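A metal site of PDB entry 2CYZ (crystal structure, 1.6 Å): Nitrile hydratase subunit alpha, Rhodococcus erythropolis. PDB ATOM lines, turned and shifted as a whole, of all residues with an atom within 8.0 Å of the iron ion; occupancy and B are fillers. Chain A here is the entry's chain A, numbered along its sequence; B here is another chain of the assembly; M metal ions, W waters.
The guanidinium group of Arg 141 of chain B lies close to SG of CSO 114.
OD of CSO 114 lies within hydrogen-bond range of the guanidinium group of Arg 56 of chain B, 2.8 Å away.
O of CSO 114 lies within hydrogen-bond range of the side-chain hydroxyl (OH) of Tyr 127 (2.7 Å).
The side-chain hydroxyl (OG) of Ser 113 lies within hydrogen-bond range of the side-chain hydroxyl (OH) of Tyr 72 of chain B (2.6 Å).
The guanidinium group of Arg 141 of chain B lies within salt-bridge range of OD2 of CSD 112 (2.9 Å).
OD1 of CSD 112 is in salt-bridge range of the guanidinium group (NE) of Arg 56 of chain B, at 2.9 Å.
O of Thr 162 lies close to SG of Cys 109, at 3.6 Å.
The backbone NH (N) of Cys 109 lies within hydrogen-bond range of the side-chain hydroxyl (OH) of Tyr 127 (3.4 Å).
The nearest printed residue that does not touch the iron ion is Arg 141 of chain B (4.7 Å).
The iron ion is bound by N of CSO 114 (2.0 Å), the backbone nitrogen of Ser 113 (2.1 Å), water W1 (2.1 Å), SG of CSD 112 (2.2 Å), SG of CSO 114 (2.2 Å) and the side-chain sulfur of Cys 109 (2.3 Å).
The iron ion has six donor atoms within binding distance.
Water W1 lies within hydrogen-bond range of the side-chain hydroxyl of Ser 113 (2.6 Å), OD of CSO 114 (2.9 Å) and OD1 of CSD 112 (2.9 Å).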
ATOM      1  N   GLN A  90     -23.367 -22.500 -20.892  1.00  0.00           N
ATOM      2  CA  GLN A  90     -22.981 -22.725 -22.290  1.00  0.00           C
ATOM      3  C   GLN A  90     -24.164 -22.433 -23.216  1.00  0.00           C
ATOM      4  O   GLN A  90     -24.320 -23.020 -24.283  1.00  0.00           O
ATOM      5  CB  GLN A  90     -22.439 -24.134 -22.504  1.00  0.00           C
ATOM      6  CG  GLN A  90     -21.153 -24.416 -21.711  1.00  0.00           C
ATOM      7  CD  GLN A  90     -20.048 -23.468 -22.165  1.00  0.00           C
ATOM      8  OE1 GLN A  90     -19.760 -23.448 -23.366  1.00  0.00           O
ATOM      9  NE2 GLN A  90     -19.460 -22.680 -21.296  1.00  0.00           N
ATOM     10  N   VAL A 108     -20.017 -26.401 -35.535  1.00  0.00           N
ATOM     11  CA  VAL A 108     -18.960 -27.251 -34.982  1.00  0.00           C
ATOM     12  C   VAL A 108     -18.240 -26.452 -33.926  1.00  0.00           C
ATOM     13  O   VAL A 108     -18.356 -25.230 -33.882  1.00  0.00           O
ATOM     14  CB  VAL A 108     -18.001 -27.708 -36.095  1.00  0.00           C
ATOM     15  CG1 VAL A 108     -17.317 -26.504 -36.759  1.00  0.00           C
ATOM     16  CG2 VAL A 108     -16.926 -28.671 -35.617  1.00  0.00           C
ATOM     17  N   CYS A 109     -17.436 -27.135 -33.105  1.00  0.00           N
ATOM     18  CA  CYS A 109     -16.377 -26.499 -32.342  1.00  0.00           C
ATOM     19  C   CYS A 109     -15.067 -27.173 -32.745  1.00  0.00           C
ATOM     20  O   CYS A 109     -14.784 -28.258 -32.219  1.00  0.00           O
ATOM     21  CB  CYS A 109     -16.649 -26.629 -30.851  1.00  0.00           C
ATOM     22  SG  CYS A 109     -15.305 -25.883 -29.837  1.00  0.00           S
ATOM     23  N   SER A 110     -14.327 -26.606 -33.684  1.00  0.00           N
ATOM     24  CA  SER A 110     -13.120 -27.342 -34.101  1.00  0.00           C
ATOM     25  C   SER A 110     -12.084 -27.434 -33.000  1.00  0.00           C
ATOM     26  O   SER A 110     -11.305 -28.405 -33.019  1.00  0.00           O
ATOM     27  CB  SER A 110     -12.501 -26.677 -35.361  1.00  0.00           C
ATOM     28  OG  SER A 110     -11.948 -25.404 -35.016  1.00  0.00           O
ATOM     29  N   LEU A 111     -12.080 -26.497 -32.041  1.00  0.00           N
ATOM     30  CA  LEU A 111     -11.043 -26.465 -31.027  1.00  0.00           C
ATOM     31  C   LEU A 111     -11.390 -27.332 -29.815  1.00  0.00           C
ATOM     32  O   LEU A 111     -10.444 -27.539 -29.019  1.00  0.00           O
ATOM     33  CB  LEU A 111     -10.822 -25.002 -30.619  1.00  0.00           C
ATOM     34  CG  LEU A 111     -10.232 -24.067 -31.674  1.00  0.00           C
ATOM     35  CD1 LEU A 111     -10.304 -22.618 -31.175  1.00  0.00           C
ATOM     36  CD2 LEU A 111      -8.797 -24.434 -32.036  1.00  0.00           C
ATOM     37  N   CSD A 112     -12.624 -27.817 -29.690  1.00  0.00           N
ATOM     38  CA  CSD A 112     -12.987 -28.635 -28.516  1.00  0.00           C
ATOM     39  CB  CSD A 112     -12.825 -27.889 -27.174  1.00  0.00           C
ATOM     40  SG  CSD A 112     -13.612 -26.234 -27.114  1.00  0.00           S
ATOM     41  C   CSD A 112     -14.411 -29.229 -28.635  1.00  0.00           C
ATOM     42  O   CSD A 112     -14.559 -30.339 -29.144  1.00  0.00           O
ATOM     43  OD1 CSD A 112     -13.425 -25.820 -25.685  1.00  0.00           O
ATOM     44  OD2 CSD A 112     -12.785 -25.406 -27.975  1.00  0.00           O
ATOM     45  N   SER A 113     -15.468 -28.542 -28.190  1.00  0.00           N
ATOM     46  CA  SER A 113     -16.786 -29.197 -28.246  1.00  0.00           C
ATOM     47  C   SER A 113     -17.948 -28.220 -28.028  1.00  0.00           C
ATOM     48  O   SER A 113     -19.104 -28.681 -27.917  1.00  0.00           O
ATOM     49  CB  SER A 113     -16.870 -30.282 -27.191  1.00  0.00           C
ATOM     50  OG  SER A 113     -16.776 -29.663 -25.895  1.00  0.00           O
ATOM     51  N   CSO A 114     -17.634 -26.949 -27.965  1.00  0.00           N
ATOM     52  CA  CSO A 114     -18.600 -25.900 -27.668  1.00  0.00           C
ATOM     53  CB  CSO A 114     -17.914 -24.586 -27.941  1.00  0.00           C
ATOM     54  SG  CSO A 114     -16.275 -24.447 -27.213  1.00  0.00           S
ATOM     55  C   CSO A 114     -19.895 -26.080 -28.480  1.00  0.00           C
ATOM     56  O   CSO A 114     -19.922 -26.256 -29.705  1.00  0.00           O
ATOM     57  OD  CSO A 114     -16.568 -24.361 -25.710  1.00  0.00           O
ATOM     58  N   THR A 115     -20.970 -26.049 -27.712  1.00  0.00           N
ATOM     59  CA  THR A 115     -22.344 -26.387 -28.024  1.00  0.00           C
ATOM     60  C   THR A 115     -23.321 -25.597 -27.157  1.00  0.00           C
ATOM     61  O   THR A 115     -23.014 -25.350 -25.987  1.00  0.00           O
ATOM     62  CB  THR A 115     -22.505 -27.878 -27.676  1.00  0.00           C
ATOM     63  OG1 THR A 115     -21.773 -28.657 -28.645  1.00  0.00           O
ATOM     64  CG2 THR A 115     -23.918 -28.389 -27.751  1.00  0.00           C
ATOM     65  N   TRP A 117     -25.565 -26.008 -24.966  1.00  0.00           N
ATOM     66  CA  TRP A 117     -26.055 -27.094 -24.125  1.00  0.00           C
ATOM     67  C   TRP A 117     -27.537 -27.040 -23.749  1.00  0.00           C
ATOM     68  O   TRP A 117     -28.217 -28.063 -23.851  1.00  0.00           O
ATOM     69  CB  TRP A 117     -25.282 -27.126 -22.822  1.00  0.00           C
ATOM     70  CG  TRP A 117     -23.856 -27.587 -22.866  1.00  0.00           C
ATOM     71  CD1 TRP A 117     -23.174 -28.128 -23.927  1.00  0.00           C
ATOM     72  CD2 TRP A 117     -22.942 -27.546 -21.766  1.00  0.00           C
ATOM     73  NE1 TRP A 117     -21.875 -28.418 -23.527  1.00  0.00           N
ATOM     74  CE2 TRP A 117     -21.718 -28.078 -22.209  1.00  0.00           C
ATOM     75  CE3 TRP A 117     -23.052 -27.112 -20.446  1.00  0.00           C
ATOM     76  CZ2 TRP A 117     -20.601 -28.175 -21.369  1.00  0.00           C
ATOM     77  CZ3 TRP A 117     -21.958 -27.208 -19.606  1.00  0.00           C
ATOM     78  CH2 TRP A 117     -20.752 -27.734 -20.061  1.00  0.00           C
ATOM     79  N   PRO A 123     -23.147 -32.141 -26.241  1.00  0.00           N
ATOM     80  CA  PRO A 123     -22.837 -32.666 -27.584  1.00  0.00           C
ATOM     81  C   PRO A 123     -22.683 -34.168 -27.568  1.00  0.00           C
ATOM     82  O   PRO A 123     -22.230 -34.753 -26.586  1.00  0.00           O
ATOM     83  CB  PRO A 123     -21.465 -32.042 -27.876  1.00  0.00           C
ATOM     84  CG  PRO A 123     -20.896 -31.639 -26.556  1.00  0.00           C
ATOM     85  CD  PRO A 123     -22.099 -31.282 -25.693  1.00  0.00           C
ATOM     86  N   TYR A 127     -19.807 -35.444 -32.462  1.00  0.00           N
ATOM     87  CA  TYR A 127     -19.547 -34.025 -32.667  1.00  0.00           C
ATOM     88  C   TYR A 127     -18.196 -33.627 -32.073  1.00  0.00           C
ATOM     89  O   TYR A 127     -17.584 -32.705 -32.591  1.00  0.00           O
ATOM     90  CB  TYR A 127     -20.661 -33.226 -32.014  1.00  0.00           C
ATOM     91  CG  TYR A 127     -20.626 -31.732 -32.008  1.00  0.00           C
ATOM     92  CD1 TYR A 127     -19.986 -31.024 -31.014  1.00  0.00           C
ATOM     93  CD2 TYR A 127     -21.273 -31.019 -33.024  1.00  0.00           C
ATOM     94  CE1 TYR A 127     -19.939 -29.636 -30.989  1.00  0.00           C
ATOM     95  CE2 TYR A 127     -21.254 -29.636 -33.010  1.00  0.00           C
ATOM     96  CZ  TYR A 127     -20.570 -28.956 -32.002  1.00  0.00           C
ATOM     97  OH  TYR A 127     -20.587 -27.568 -31.983  1.00  0.00           O
ATOM     98  N   LYS A 128     -17.806 -34.327 -31.015  1.00  0.00           N
ATOM     99  CA  LYS A 128     -16.540 -34.102 -30.346  1.00  0.00           C
ATOM    100  C   LYS A 128     -15.408 -34.906 -30.988  1.00  0.00           C
ATOM    101  O   LYS A 128     -14.246 -34.765 -30.573  1.00  0.00           O
ATOM    102  CB  LYS A 128     -16.706 -34.458 -28.858  1.00  0.00           C
ATOM    103  CG  LYS A 128     -17.776 -33.626 -28.164  1.00  0.00           C
ATOM    104  CD  LYS A 128     -17.965 -34.053 -26.720  1.00  0.00           C
ATOM    105  CE  LYS A 128     -18.858 -35.248 -26.558  1.00  0.00           C
ATOM    106  NZ  LYS A 128     -19.226 -35.573 -25.150  1.00  0.00           N
ATOM    107  N   ARG A 133     -14.308 -32.565 -36.086  1.00  0.00           N
ATOM    108  CA  ARG A 133     -13.569 -31.349 -35.805  1.00  0.00           C
ATOM    109  C   ARG A 133     -12.581 -30.964 -36.878  1.00  0.00           C
ATOM    110  O   ARG A 133     -12.366 -29.785 -37.164  1.00  0.00           O
ATOM    111  CB  ARG A 133     -12.819 -31.489 -34.449  1.00  0.00           C
ATOM    112  CG  ARG A 133     -13.841 -31.515 -33.317  1.00  0.00           C
ATOM    113  CD  ARG A 133     -13.244 -31.631 -31.912  1.00  0.00           C
ATOM    114  NE  ARG A 133     -12.046 -30.818 -31.732  1.00  0.00           N
ATOM    115  CZ  ARG A 133     -11.027 -31.073 -30.934  1.00  0.00           C
ATOM    116  NH1 ARG A 133     -10.991 -32.128 -30.117  1.00  0.00           N
ATOM    117  NH2 ARG A 133     -10.006 -30.199 -30.942  1.00  0.00           N
ATOM    118  N   ASP A 161     -17.944 -22.009 -36.795  1.00  0.00           N
ATOM    119  CA  ASP A 161     -17.031 -22.616 -35.813  1.00  0.00           C
ATOM    120  C   ASP A 161     -17.189 -21.884 -34.481  1.00  0.00           C
ATOM    121  O   ASP A 161     -16.972 -20.665 -34.397  1.00  0.00           O
ATOM    122  CB  ASP A 161     -15.618 -22.517 -36.390  1.00  0.00           C
ATOM    123  CG  ASP A 161     -14.621 -23.412 -35.662  1.00  0.00           C
ATOM    124  OD1 ASP A 161     -14.951 -23.999 -34.623  1.00  0.00           O
ATOM    125  OD2 ASP A 161     -13.480 -23.491 -36.127  1.00  0.00           O
ATOM    126  N   THR A 162     -17.606 -22.624 -33.456  1.00  0.00           N
ATOM    127  CA  THR A 162     -17.957 -22.009 -32.162  1.00  0.00           C
ATOM    128  C   THR A 162     -16.692 -21.742 -31.341  1.00  0.00           C
ATOM    129  O   THR A 162     -16.350 -22.529 -30.457  1.00  0.00           O
ATOM    130  CB  THR A 162     -18.908 -22.951 -31.407  1.00  0.00           C
ATOM    131  OG1 THR A 162     -20.030 -23.287 -32.255  1.00  0.00           O
ATOM    132  CG2 THR A 162     -19.435 -22.289 -30.126  1.00  0.00           C
ATOM    133  N   THR A 163     -16.008 -20.653 -31.645  1.00  0.00           N
ATOM    134  CA  THR A 163     -14.691 -20.354 -31.084  1.00  0.00           C
ATOM    135  C   THR A 163     -14.727 -19.380 -29.925  1.00  0.00           C
ATOM    136  O   THR A 163     -13.688 -19.156 -29.317  1.00  0.00           O
ATOM    137  CB  THR A 163     -13.806 -19.741 -32.193  1.00  0.00           C
ATOM    138  OG1 THR A 163     -14.560 -18.752 -32.921  1.00  0.00           O
ATOM    139  CG2 THR A 163     -13.422 -20.807 -33.225  1.00  0.00           C
ATOM    140  N   ALA A 164     -15.911 -18.787 -29.613  1.00  0.00           N
ATOM    141  CA  ALA A 164     -15.915 -17.856 -28.464  1.00  0.00           C
ATOM    142  C   ALA A 164     -17.159 -18.115 -27.631  1.00  0.00           C
ATOM    143  O   ALA A 164     -17.378 -19.267 -27.262  1.00  0.00           O
ATOM    144  CB  ALA A 164     -15.741 -16.438 -28.977  1.00  0.00           C
ATOM    145  N   ARG A 167     -23.308 -19.091 -28.821  1.00  0.00           N
ATOM    146  CA  ARG A 167     -23.724 -20.497 -28.866  1.00  0.00           C
ATOM    147  C   ARG A 167     -24.849 -20.582 -29.879  1.00  0.00           C
ATOM    148  O   ARG A 167     -25.823 -19.794 -29.834  1.00  0.00           O
ATOM    149  CB  ARG A 167     -24.141 -20.961 -27.462  1.00  0.00           C
ATOM    150  CG  ARG A 167     -22.922 -21.043 -26.530  1.00  0.00           C
ATOM    151  CD  ARG A 167     -22.048 -22.270 -26.843  1.00  0.00           C
ATOM    152  NE  ARG A 167     -20.857 -22.275 -25.959  1.00  0.00           N
ATOM    153  CZ  ARG A 167     -19.767 -21.533 -26.169  1.00  0.00           C
ATOM    154  NH1 ARG A 167     -19.711 -20.743 -27.238  1.00  0.00           N
ATOM    155  NH2 ARG A 167     -18.727 -21.576 -25.324  1.00  0.00           N
ATOM    156  N   TYR B  37     -17.237 -32.357 -15.945  1.00  0.00           N
ATOM    157  CA  TYR B  37     -17.942 -31.084 -16.059  1.00  0.00           C
ATOM    158  C   TYR B  37     -18.388 -30.601 -14.681  1.00  0.00           C
ATOM    159  O   TYR B  37     -18.270 -29.417 -14.384  1.00  0.00           O
ATOM    160  CB  TYR B  37     -19.169 -31.280 -16.954  1.00  0.00           C
ATOM    161  CG  TYR B  37     -18.925 -31.282 -18.455  1.00  0.00           C
ATOM    162  CD1 TYR B  37     -17.651 -31.128 -19.007  1.00  0.00           C
ATOM    163  CD2 TYR B  37     -20.024 -31.413 -19.288  1.00  0.00           C
ATOM    164  CE1 TYR B  37     -17.518 -31.124 -20.388  1.00  0.00           C
ATOM    165  CE2 TYR B  37     -19.882 -31.408 -20.666  1.00  0.00           C
ATOM    166  CZ  TYR B  37     -18.614 -31.275 -21.195  1.00  0.00           C
ATOM    167  OH  TYR B  37     -18.512 -31.263 -22.584  1.00  0.00           O
ATOM    168  N   ARG B  56     -10.064 -24.935 -20.877  1.00  0.00           N
ATOM    169  CA  ARG B  56      -9.734 -25.187 -22.286  1.00  0.00           C
ATOM    170  C   ARG B  56      -8.210 -25.251 -22.456  1.00  0.00           C
ATOM    171  O   ARG B  56      -7.728 -26.157 -23.143  1.00  0.00           O
ATOM    172  CB  ARG B  56     -10.315 -24.133 -23.208  1.00  0.00           C
ATOM    173  CG  ARG B  56     -11.846 -24.087 -23.208  1.00  0.00           C
ATOM    174  CD  ARG B  56     -12.295 -23.141 -24.366  1.00  0.00           C
ATOM    175  NE  ARG B  56     -13.770 -23.206 -24.374  1.00  0.00           N
ATOM    176  CZ  ARG B  56     -14.514 -22.312 -23.708  1.00  0.00           C
ATOM    177  NH1 ARG B  56     -13.938 -21.327 -23.039  1.00  0.00           N
ATOM    178  NH2 ARG B  56     -15.832 -22.473 -23.769  1.00  0.00           N
ATOM    179  N   TYR B  72     -12.614 -37.930 -25.047  1.00  0.00           N
ATOM    180  CA  TYR B  72     -13.043 -36.600 -24.640  1.00  0.00           C
ATOM    181  C   TYR B  72     -13.185 -36.419 -23.120  1.00  0.00           C
ATOM    182  O   TYR B  72     -12.518 -35.576 -22.511  1.00  0.00           O
ATOM    183  CB  TYR B  72     -14.393 -36.298 -25.363  1.00  0.00           C
ATOM    184  CG  TYR B  72     -14.903 -34.918 -24.937  1.00  0.00           C
ATOM    185  CD1 TYR B  72     -14.474 -33.777 -25.589  1.00  0.00           C
ATOM    186  CD2 TYR B  72     -15.839 -34.757 -23.913  1.00  0.00           C
ATOM    187  CE1 TYR B  72     -14.932 -32.524 -25.238  1.00  0.00           C
ATOM    188  CE2 TYR B  72     -16.278 -33.498 -23.531  1.00  0.00           C
ATOM    189  CZ  TYR B  72     -15.820 -32.393 -24.184  1.00  0.00           C
ATOM    190  OH  TYR B  72     -16.285 -31.122 -23.823  1.00  0.00           O
ATOM    191  N   TYR B  76     -10.922 -34.110 -19.814  1.00  0.00           N
ATOM    192  CA  TYR B  76     -11.335 -33.113 -18.843  1.00  0.00           C
ATOM    193  C   TYR B  76     -11.099 -33.601 -17.431  1.00  0.00           C
ATOM    194  O   TYR B  76     -10.893 -32.757 -16.557  1.00  0.00           O
ATOM    195  CB  TYR B  76     -12.830 -32.682 -19.056  1.00  0.00           C
ATOM    196  CG  TYR B  76     -12.773 -31.870 -20.366  1.00  0.00           C
ATOM    197  CD1 TYR B  76     -12.574 -30.502 -20.444  1.00  0.00           C
ATOM    198  CD2 TYR B  76     -12.891 -32.578 -21.558  1.00  0.00           C
ATOM    199  CE1 TYR B  76     -12.510 -29.849 -21.667  1.00  0.00           C
ATOM    200  CE2 TYR B  76     -12.819 -31.941 -22.768  1.00  0.00           C
ATOM    201  CZ  TYR B  76     -12.643 -30.580 -22.840  1.00  0.00           C
ATOM    202  OH  TYR B  76     -12.561 -29.985 -24.083  1.00  0.00           O
ATOM    203  N   ARG B 141      -8.179 -18.132 -28.853  1.00  0.00           N
ATOM    204  CA  ARG B 141      -9.377 -18.716 -29.476  1.00  0.00           C
ATOM    205  C   ARG B 141      -9.460 -18.319 -30.934  1.00  0.00           C
ATOM    206  O   ARG B 141     -10.448 -17.863 -31.483  1.00  0.00           O
ATOM    207  CB  ARG B 141     -10.609 -18.207 -28.693  1.00  0.00           C
ATOM    208  CG  ARG B 141     -10.661 -18.786 -27.281  1.00  0.00           C
ATOM    209  CD  ARG B 141     -10.615 -20.320 -27.311  1.00  0.00           C
ATOM    210  NE  ARG B 141     -11.874 -20.855 -27.854  1.00  0.00           N
ATOM    211  CZ  ARG B 141     -12.104 -22.167 -28.002  1.00  0.00           C
ATOM    212  NH1 ARG B 141     -11.159 -23.042 -27.680  1.00  0.00           N
ATOM    213  NH2 ARG B 141     -13.260 -22.594 -28.470  1.00  0.00           N
HETATM  214 FE    FE M   1     -15.689 -26.548 -27.699  1.00  0.00          FE
HETATM  215  O   HOH W   1     -16.011 -27.164 -25.713  1.00  0.00           O
